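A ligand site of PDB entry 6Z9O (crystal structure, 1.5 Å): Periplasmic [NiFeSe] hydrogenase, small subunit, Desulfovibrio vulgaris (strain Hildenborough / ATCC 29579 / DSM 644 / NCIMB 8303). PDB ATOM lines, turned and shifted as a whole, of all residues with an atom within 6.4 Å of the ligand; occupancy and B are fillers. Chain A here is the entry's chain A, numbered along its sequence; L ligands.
The backbone NH of His 208 is in hydrogen-bond range of the backbone carbonyl oxygen of Gly 240 (3.3 Å). SG of Cys 211 sits close to N of Tyr 213, 3.4 Å away. The side-chain sulfur of Cys 232 sits close to the backbone NH of Tyr 234, at 3.3 Å. SD of Met 222 sits close to SG of Cys 232. The backbone NH (N) of Cys 238 sits at hydrogen-bond distance from the backbone carbonyl oxygen (O) of Arg 233, 3.2 Å away. The guanidinium group (NE) of Arg 233 lies within hydrogen-bond range of the backbone carbonyl oxygen (O) of Val 260, 2.8 Å away. NH2 of Arg 233 sits at hydrogen-bond distance from OH of Tyr 213 (3.2 Å). The guanidinium group (NH1) of Arg 233 is in hydrogen-bond range of the backbone carbonyl oxygen (O) of Gly 231 (2.8 Å).
The backbone carbonyl oxygen (O) of Tyr 213 sits close to a sulfur (S1) of the ligand, at 3.7 Å. CB of Tyr 217 touches S1 of the ligand, 3.8 Å away. CB of Tyr 234 touches S4 of the ligand, 3.7 Å away. Gly 240 touches the ligand (CA to S3, 3.8 Å). CD of Pro 241 touches S4 of the ligand (3.99 Å). Val 260 touches the ligand. Hydrophobic or aromatic side chains within 4 Å of the ligand: His 208, Tyr 217, Tyr 234, Pro 241 and Val 260. 12 residues have an atom within 4 Å of the ligand: His 208, Cys 211, Tyr 213, Leu 214, Tyr 217, Cys 232, Arg 233, Tyr 234, Cys 238, Gly 240, Pro 241 and Val 260.
A ring nitrogen (ND1) of His 208 binds an iron atom (FE2) of the ligand (2.1 Å). FE4 of the ligand is bound by SG of Cys 211 (2.3 Å). The side-chain sulfur of Cys 232 is bound to an iron atom (FE3) of the ligand (2.3 Å). The side-chain sulfur of Cys 238 binds an iron atom (FE1) of the ligand (2.3 Å). The backbone NH of Arg 233 sits close to a sulfur (S2) of the ligand, 3.5 Å away. The backbone NH (N) of Leu 214 sits close to a sulfur (S1) of the ligand (3.7 Å).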
ATOM      1  N   ILE A 207      -7.891  11.144  25.883  1.00  0.00           N
ATOM      2  CA  ILE A 207      -8.765  10.431  26.812  1.00  0.00           C
ATOM      3  C   ILE A 207      -9.297   9.160  26.180  1.00  0.00           C
ATOM      4  O   ILE A 207      -9.202   8.065  26.751  1.00  0.00           O
ATOM      5  CB  ILE A 207      -9.922  11.344  27.274  1.00  0.00           C
ATOM      6  CG1 ILE A 207      -9.387  12.473  28.160  1.00  0.00           C
ATOM      7  CG2 ILE A 207     -11.011  10.518  27.997  1.00  0.00           C
ATOM      8  CD1 ILE A 207     -10.429  13.189  28.959  1.00  0.00           C
ATOM      9  N   HIS A 208      -9.886   9.295  24.991  1.00  0.00           N
ATOM     10  CA  HIS A 208     -10.592   8.171  24.374  1.00  0.00           C
ATOM     11  C   HIS A 208      -9.648   7.016  24.069  1.00  0.00           C
ATOM     12  O   HIS A 208      -9.975   5.850  24.332  1.00  0.00           O
ATOM     13  CB  HIS A 208     -11.297   8.695  23.106  1.00  0.00           C
ATOM     14  CG  HIS A 208     -11.800   7.634  22.177  1.00  0.00           C
ATOM     15  ND1 HIS A 208     -13.027   7.022  22.331  1.00  0.00           N
ATOM     16  CD2 HIS A 208     -11.279   7.139  21.033  1.00  0.00           C
ATOM     17  CE1 HIS A 208     -13.220   6.170  21.348  1.00  0.00           C
ATOM     18  NE2 HIS A 208     -12.171   6.221  20.538  1.00  0.00           N
ATOM     19  N   GLU A 209      -8.448   7.316  23.549  1.00  0.00           N
ATOM     20  CA  GLU A 209      -7.514   6.255  23.192  1.00  0.00           C
ATOM     21  C   GLU A 209      -7.037   5.474  24.409  1.00  0.00           C
ATOM     22  O   GLU A 209      -6.537   4.350  24.243  1.00  0.00           O
ATOM     23  CB  GLU A 209      -6.323   6.843  22.450  1.00  0.00           C
ATOM     24  CG  GLU A 209      -6.690   7.461  21.118  1.00  0.00           C
ATOM     25  CD  GLU A 209      -7.229   6.439  20.137  1.00  0.00           C
ATOM     26  OE1 GLU A 209      -6.617   5.366  19.987  1.00  0.00           O
ATOM     27  OE2 GLU A 209      -8.280   6.712  19.525  1.00  0.00           O
ATOM     28  N   CYS A 211      -9.193   5.082  27.163  1.00  0.00           N
ATOM     29  CA  CYS A 211     -10.413   4.974  27.953  1.00  0.00           C
ATOM     30  C   CYS A 211     -10.722   3.512  28.282  1.00  0.00           C
ATOM     31  O   CYS A 211     -10.624   2.640  27.403  1.00  0.00           O
ATOM     32  CB  CYS A 211     -11.594   5.577  27.210  1.00  0.00           C
ATOM     33  SG  CYS A 211     -13.141   5.513  28.145  1.00  0.00           S
ATOM     34  N   PRO A 212     -11.135   3.211  29.514  1.00  0.00           N
ATOM     35  CA  PRO A 212     -11.502   1.824  29.843  1.00  0.00           C
ATOM     36  C   PRO A 212     -12.688   1.294  29.070  1.00  0.00           C
ATOM     37  O   PRO A 212     -12.861   0.071  28.999  1.00  0.00           O
ATOM     38  CB  PRO A 212     -11.813   1.893  31.350  1.00  0.00           C
ATOM     39  CG  PRO A 212     -12.121   3.304  31.622  1.00  0.00           C
ATOM     40  CD  PRO A 212     -11.262   4.098  30.684  1.00  0.00           C
ATOM     41  N   TYR A 213     -13.529   2.152  28.498  1.00  0.00           N
ATOM     42  CA  TYR A 213     -14.684   1.685  27.737  1.00  0.00           C
ATOM     43  C   TYR A 213     -14.414   1.646  26.238  1.00  0.00           C
ATOM     44  O   TYR A 213     -15.357   1.496  25.447  1.00  0.00           O
ATOM     45  CB  TYR A 213     -15.899   2.551  28.051  1.00  0.00           C
ATOM     46  CG  TYR A 213     -16.077   2.750  29.548  1.00  0.00           C
ATOM     47  CD1 TYR A 213     -16.481   1.702  30.375  1.00  0.00           C
ATOM     48  CD2 TYR A 213     -15.816   3.982  30.132  1.00  0.00           C
ATOM     49  CE1 TYR A 213     -16.637   1.889  31.749  1.00  0.00           C
ATOM     50  CE2 TYR A 213     -15.967   4.175  31.499  1.00  0.00           C
ATOM     51  CZ  TYR A 213     -16.367   3.129  32.302  1.00  0.00           C
ATOM     52  OH  TYR A 213     -16.498   3.368  33.661  1.00  0.00           O
ATOM     53  N   LEU A 214     -13.146   1.751  25.822  1.00  0.00           N
ATOM     54  CA  LEU A 214     -12.839   1.733  24.393  1.00  0.00           C
ATOM     55  C   LEU A 214     -13.231   0.408  23.749  1.00  0.00           C
ATOM     56  O   LEU A 214     -13.606   0.380  22.575  1.00  0.00           O
ATOM     57  CB  LEU A 214     -11.332   2.006  24.185  1.00  0.00           C
ATOM     58  CG  LEU A 214     -10.843   2.249  22.750  1.00  0.00           C
ATOM     59  CD1 LEU A 214     -11.458   3.507  22.132  1.00  0.00           C
ATOM     60  CD2 LEU A 214      -9.324   2.359  22.729  1.00  0.00           C
ATOM     61  N   ASP A 215     -13.189  -0.695  24.505  1.00  0.00           N
ATOM     62  CA  ASP A 215     -13.622  -1.969  23.941  1.00  0.00           C
ATOM     63  C   ASP A 215     -15.096  -1.919  23.567  1.00  0.00           C
ATOM     64  O   ASP A 215     -15.490  -2.452  22.521  1.00  0.00           O
ATOM     65  CB  ASP A 215     -13.324  -3.107  24.924  1.00  0.00           C
ATOM     66  CG  ASP A 215     -14.058  -2.966  26.257  1.00  0.00           C
ATOM     67  OD1 ASP A 215     -14.298  -1.830  26.717  1.00  0.00           O
ATOM     68  OD2 ASP A 215     -14.391  -4.025  26.854  1.00  0.00           O
ATOM     69  N   LYS A 216     -15.918  -1.276  24.395  1.00  0.00           N
ATOM     70  CA  LYS A 216     -17.337  -1.138  24.068  1.00  0.00           C
ATOM     71  C   LYS A 216     -17.533  -0.209  22.873  1.00  0.00           C
ATOM     72  O   LYS A 216     -18.392  -0.455  22.026  1.00  0.00           O
ATOM     73  CB  LYS A 216     -18.110  -0.620  25.281  1.00  0.00           C
ATOM     74  CG  LYS A 216     -18.013  -1.522  26.498  1.00  0.00           C
ATOM     75  CD  LYS A 216     -18.560  -2.925  26.202  1.00  0.00           C
ATOM     76  CE  LYS A 216     -18.414  -3.838  27.402  1.00  0.00           C
ATOM     77  NZ  LYS A 216     -18.665  -5.248  27.009  1.00  0.00           N
ATOM     78  N   TYR A 217     -16.735   0.866  22.803  1.00  0.00           N
ATOM     79  CA  TYR A 217     -16.768   1.730  21.632  1.00  0.00           C
ATOM     80  C   TYR A 217     -16.487   0.931  20.363  1.00  0.00           C
ATOM     81  O   TYR A 217     -17.237   1.008  19.390  1.00  0.00           O
ATOM     82  CB  TYR A 217     -15.762   2.859  21.791  1.00  0.00           C
ATOM     83  CG  TYR A 217     -15.682   3.781  20.599  1.00  0.00           C
ATOM     84  CD1 TYR A 217     -16.484   4.914  20.516  1.00  0.00           C
ATOM     85  CD2 TYR A 217     -14.799   3.525  19.558  1.00  0.00           C
ATOM     86  CE1 TYR A 217     -16.411   5.763  19.438  1.00  0.00           C
ATOM     87  CE2 TYR A 217     -14.719   4.371  18.468  1.00  0.00           C
ATOM     88  CZ  TYR A 217     -15.527   5.488  18.411  1.00  0.00           C
ATOM     89  OH  TYR A 217     -15.459   6.333  17.340  1.00  0.00           O
ATOM     90  N   MET A 222     -23.261   0.830  23.051  1.00  0.00           N
ATOM     91  CA  MET A 222     -23.451   2.201  23.520  1.00  0.00           C
ATOM     92  C   MET A 222     -24.528   2.253  24.587  1.00  0.00           C
ATOM     93  O   MET A 222     -25.597   1.658  24.422  1.00  0.00           O
ATOM     94  CB  MET A 222     -23.856   3.138  22.383  1.00  0.00           C
ATOM     95  CG  MET A 222     -22.853   3.272  21.273  1.00  0.00           C
ATOM     96  SD  MET A 222     -21.343   4.044  21.866  1.00  0.00           S
ATOM     97  CE  MET A 222     -20.273   3.756  20.460  1.00  0.00           C
ATOM     98  N   GLY A 231     -22.011   0.247  28.755  1.00  0.00           N
ATOM     99  CA  GLY A 231     -21.713   0.706  27.416  1.00  0.00           C
ATOM    100  C   GLY A 231     -20.759   1.877  27.370  1.00  0.00           C
ATOM    101  O   GLY A 231     -20.439   2.516  28.370  1.00  0.00           O
ATOM    102  N   CYS A 232     -20.285   2.142  26.155  1.00  0.00           N
ATOM    103  CA  CYS A 232     -19.578   3.381  25.870  1.00  0.00           C
ATOM    104  C   CYS A 232     -20.555   4.552  25.921  1.00  0.00           C
ATOM    105  O   CYS A 232     -21.742   4.408  25.649  1.00  0.00           O
ATOM    106  CB  CYS A 232     -18.903   3.286  24.501  1.00  0.00           C
ATOM    107  SG  CYS A 232     -18.331   4.828  23.773  1.00  0.00           S
ATOM    108  N   ARG A 233     -20.020   5.723  26.295  1.00  0.00           N
ATOM    109  CA  ARG A 233     -20.785   6.944  26.517  1.00  0.00           C
ATOM    110  C   ARG A 233     -20.883   7.843  25.283  1.00  0.00           C
ATOM    111  O   ARG A 233     -21.370   8.976  25.394  1.00  0.00           O
ATOM    112  CB  ARG A 233     -20.157   7.748  27.658  1.00  0.00           C
ATOM    113  CG  ARG A 233     -20.393   7.229  29.082  1.00  0.00           C
ATOM    114  CD  ARG A 233     -19.753   5.881  29.392  1.00  0.00           C
ATOM    115  NE  ARG A 233     -19.579   5.729  30.834  1.00  0.00           N
ATOM    116  CZ  ARG A 233     -19.510   4.567  31.494  1.00  0.00           C
ATOM    117  NH1 ARG A 233     -19.596   3.420  30.854  1.00  0.00           N
ATOM    118  NH2 ARG A 233     -19.353   4.570  32.809  1.00  0.00           N
ATOM    119  N   TYR A 234     -20.454   7.366  24.116  1.00  0.00           N
ATOM    120  CA  TYR A 234     -20.356   8.247  22.949  1.00  0.00           C
ATOM    121  C   TYR A 234     -21.725   8.774  22.531  1.00  0.00           C
ATOM    122  O   TYR A 234     -21.876   9.978  22.260  1.00  0.00           O
ATOM    123  CB  TYR A 234     -19.705   7.483  21.796  1.00  0.00           C
ATOM    124  CG  TYR A 234     -19.542   8.283  20.530  1.00  0.00           C
ATOM    125  CD1 TYR A 234     -18.429   9.088  20.339  1.00  0.00           C
ATOM    126  CD2 TYR A 234     -20.488   8.223  19.517  1.00  0.00           C
ATOM    127  CE1 TYR A 234     -18.273   9.813  19.168  1.00  0.00           C
ATOM    128  CE2 TYR A 234     -20.346   8.943  18.348  1.00  0.00           C
ATOM    129  CZ  TYR A 234     -19.234   9.738  18.177  1.00  0.00           C
ATOM    130  OH  TYR A 234     -19.097  10.453  17.015  1.00  0.00           O
ATOM    131  N   ASP A 235     -22.730   7.908  22.454  1.00  0.00           N
ATOM    132  CA  ASP A 235     -24.044   8.366  22.023  1.00  0.00           C
ATOM    133  C   ASP A 235     -24.664   9.329  23.016  1.00  0.00           C
ATOM    134  O   ASP A 235     -25.530  10.125  22.638  1.00  0.00           O
ATOM    135  CB  ASP A 235     -24.990   7.178  21.791  1.00  0.00           C
ATOM    136  CG  ASP A 235     -24.695   6.436  20.488  1.00  0.00           C
ATOM    137  OD1 ASP A 235     -23.874   6.943  19.698  1.00  0.00           O
ATOM    138  OD2 ASP A 235     -25.291   5.368  20.263  1.00  0.00           O
ATOM    139  N   CYS A 238     -20.263  11.905  24.871  1.00  0.00           N
ATOM    140  CA  CYS A 238     -18.884  11.923  25.371  1.00  0.00           C
ATOM    141  C   CYS A 238     -17.933  12.525  24.342  1.00  0.00           C
ATOM    142  O   CYS A 238     -17.898  12.092  23.186  1.00  0.00           O
ATOM    143  CB  CYS A 238     -18.436  10.509  25.712  1.00  0.00           C
ATOM    144  SG  CYS A 238     -16.799  10.454  26.468  1.00  0.00           S
ATOM    145  N   LYS A 239     -17.151  13.513  24.769  1.00  0.00           N
ATOM    146  CA  LYS A 239     -16.195  14.213  23.916  1.00  0.00           C
ATOM    147  C   LYS A 239     -14.763  13.722  24.119  1.00  0.00           C
ATOM    148  O   LYS A 239     -13.812  14.380  23.661  1.00  0.00           O
ATOM    149  CB  LYS A 239     -16.272  15.726  24.155  1.00  0.00           C
ATOM    150  CG  LYS A 239     -17.669  16.303  23.941  1.00  0.00           C
ATOM    151  CD  LYS A 239     -18.154  16.037  22.527  1.00  0.00           C
ATOM    152  CE  LYS A 239     -19.409  16.804  22.168  1.00  0.00           C
ATOM    153  NZ  LYS A 239     -20.545  16.399  22.998  1.00  0.00           N
ATOM    154  N   GLY A 240     -14.580  12.580  24.789  1.00  0.00           N
ATOM    155  CA  GLY A 240     -13.262  12.000  24.960  1.00  0.00           C
ATOM    156  C   GLY A 240     -12.434  11.873  23.703  1.00  0.00           C
ATOM    157  O   GLY A 240     -11.208  12.036  23.759  1.00  0.00           O
ATOM    158  N   PRO A 241     -13.043  11.556  22.537  1.00  0.00           N
ATOM    159  CA  PRO A 241     -12.244  11.453  21.307  1.00  0.00           C
ATOM    160  C   PRO A 241     -11.453  12.698  20.971  1.00  0.00           C
ATOM    161  O   PRO A 241     -10.372  12.580  20.373  1.00  0.00           O
ATOM    162  CB  PRO A 241     -13.298  11.158  20.229  1.00  0.00           C
ATOM    163  CG  PRO A 241     -14.363  10.430  20.956  1.00  0.00           C
ATOM    164  CD  PRO A 241     -14.412  11.046  22.337  1.00  0.00           C
ATOM    165  N   TRP A 258     -14.549   9.931  37.991  1.00  0.00           N
ATOM    166  CA  TRP A 258     -14.210  10.866  36.935  1.00  0.00           C
ATOM    167  C   TRP A 258     -15.386  10.994  35.985  1.00  0.00           C
ATOM    168  O   TRP A 258     -16.355  10.238  36.056  1.00  0.00           O
ATOM    169  CB  TRP A 258     -12.917  10.472  36.209  1.00  0.00           C
ATOM    170  CG  TRP A 258     -12.945   9.228  35.409  1.00  0.00           C
ATOM    171  CD1 TRP A 258     -13.228   7.972  35.852  1.00  0.00           C
ATOM    172  CD2 TRP A 258     -12.628   9.091  34.013  1.00  0.00           C
ATOM    173  NE1 TRP A 258     -13.124   7.064  34.821  1.00  0.00           N
ATOM    174  CE2 TRP A 258     -12.762   7.732  33.683  1.00  0.00           C
ATOM    175  CE3 TRP A 258     -12.248   9.995  33.020  1.00  0.00           C
ATOM    176  CZ2 TRP A 258     -12.526   7.248  32.388  1.00  0.00           C
ATOM    177  CZ3 TRP A 258     -12.019   9.514  31.737  1.00  0.00           C
ATOM    178  CH2 TRP A 258     -12.149   8.153  31.436  1.00  0.00           C
ATOM    179  N   VAL A 260     -16.140  10.483  32.839  1.00  0.00           N
ATOM    180  CA  VAL A 260     -16.633   9.460  31.932  1.00  0.00           C
ATOM    181  C   VAL A 260     -17.311   8.335  32.695  1.00  0.00           C
ATOM    182  O   VAL A 260     -18.328   7.788  32.243  1.00  0.00           O
ATOM    183  CB  VAL A 260     -15.491   8.937  31.048  1.00  0.00           C
ATOM    184  CG1 VAL A 260     -15.960   7.751  30.222  1.00  0.00           C
ATOM    185  CG2 VAL A 260     -14.951  10.055  30.168  1.00  0.00           C
ATOM    186  N   CYS A 265     -17.500  12.971  29.360  1.00  0.00           N
ATOM    187  CA  CYS A 265     -16.501  14.019  29.240  1.00  0.00           C
ATOM    188  C   CYS A 265     -17.040  15.114  28.327  1.00  0.00           C
ATOM    189  O   CYS A 265     -17.660  14.826  27.303  1.00  0.00           O
ATOM    190  CB  CYS A 265     -15.190  13.444  28.693  1.00  0.00           C
ATOM    191  SG  CYS A 265     -13.902  14.628  28.263  1.00  0.00           S
HETATM  192 FE1  LIG L   1     -16.034   8.407  25.761  1.00  0.00          FE
HETATM  193 FE2  LIG L   1     -14.309   7.169  23.970  1.00  0.00          FE
HETATM  194 FE3  LIG L   1     -16.574   5.893  24.745  1.00  0.00          FE
HETATM  195 FE4  LIG L   1     -14.490   6.259  26.502  1.00  0.00          FE
HETATM  196  S1  LIG L   1     -14.475   4.966  24.622  1.00  0.00           S
HETATM  197  S2  LIG L   1     -16.726   6.560  26.937  1.00  0.00           S
HETATM  198  S3  LIG L   1     -13.753   8.336  25.858  1.00  0.00           S
HETATM  199  S4  LIG L   1     -16.473   7.865  23.574  1.00  0.00           S
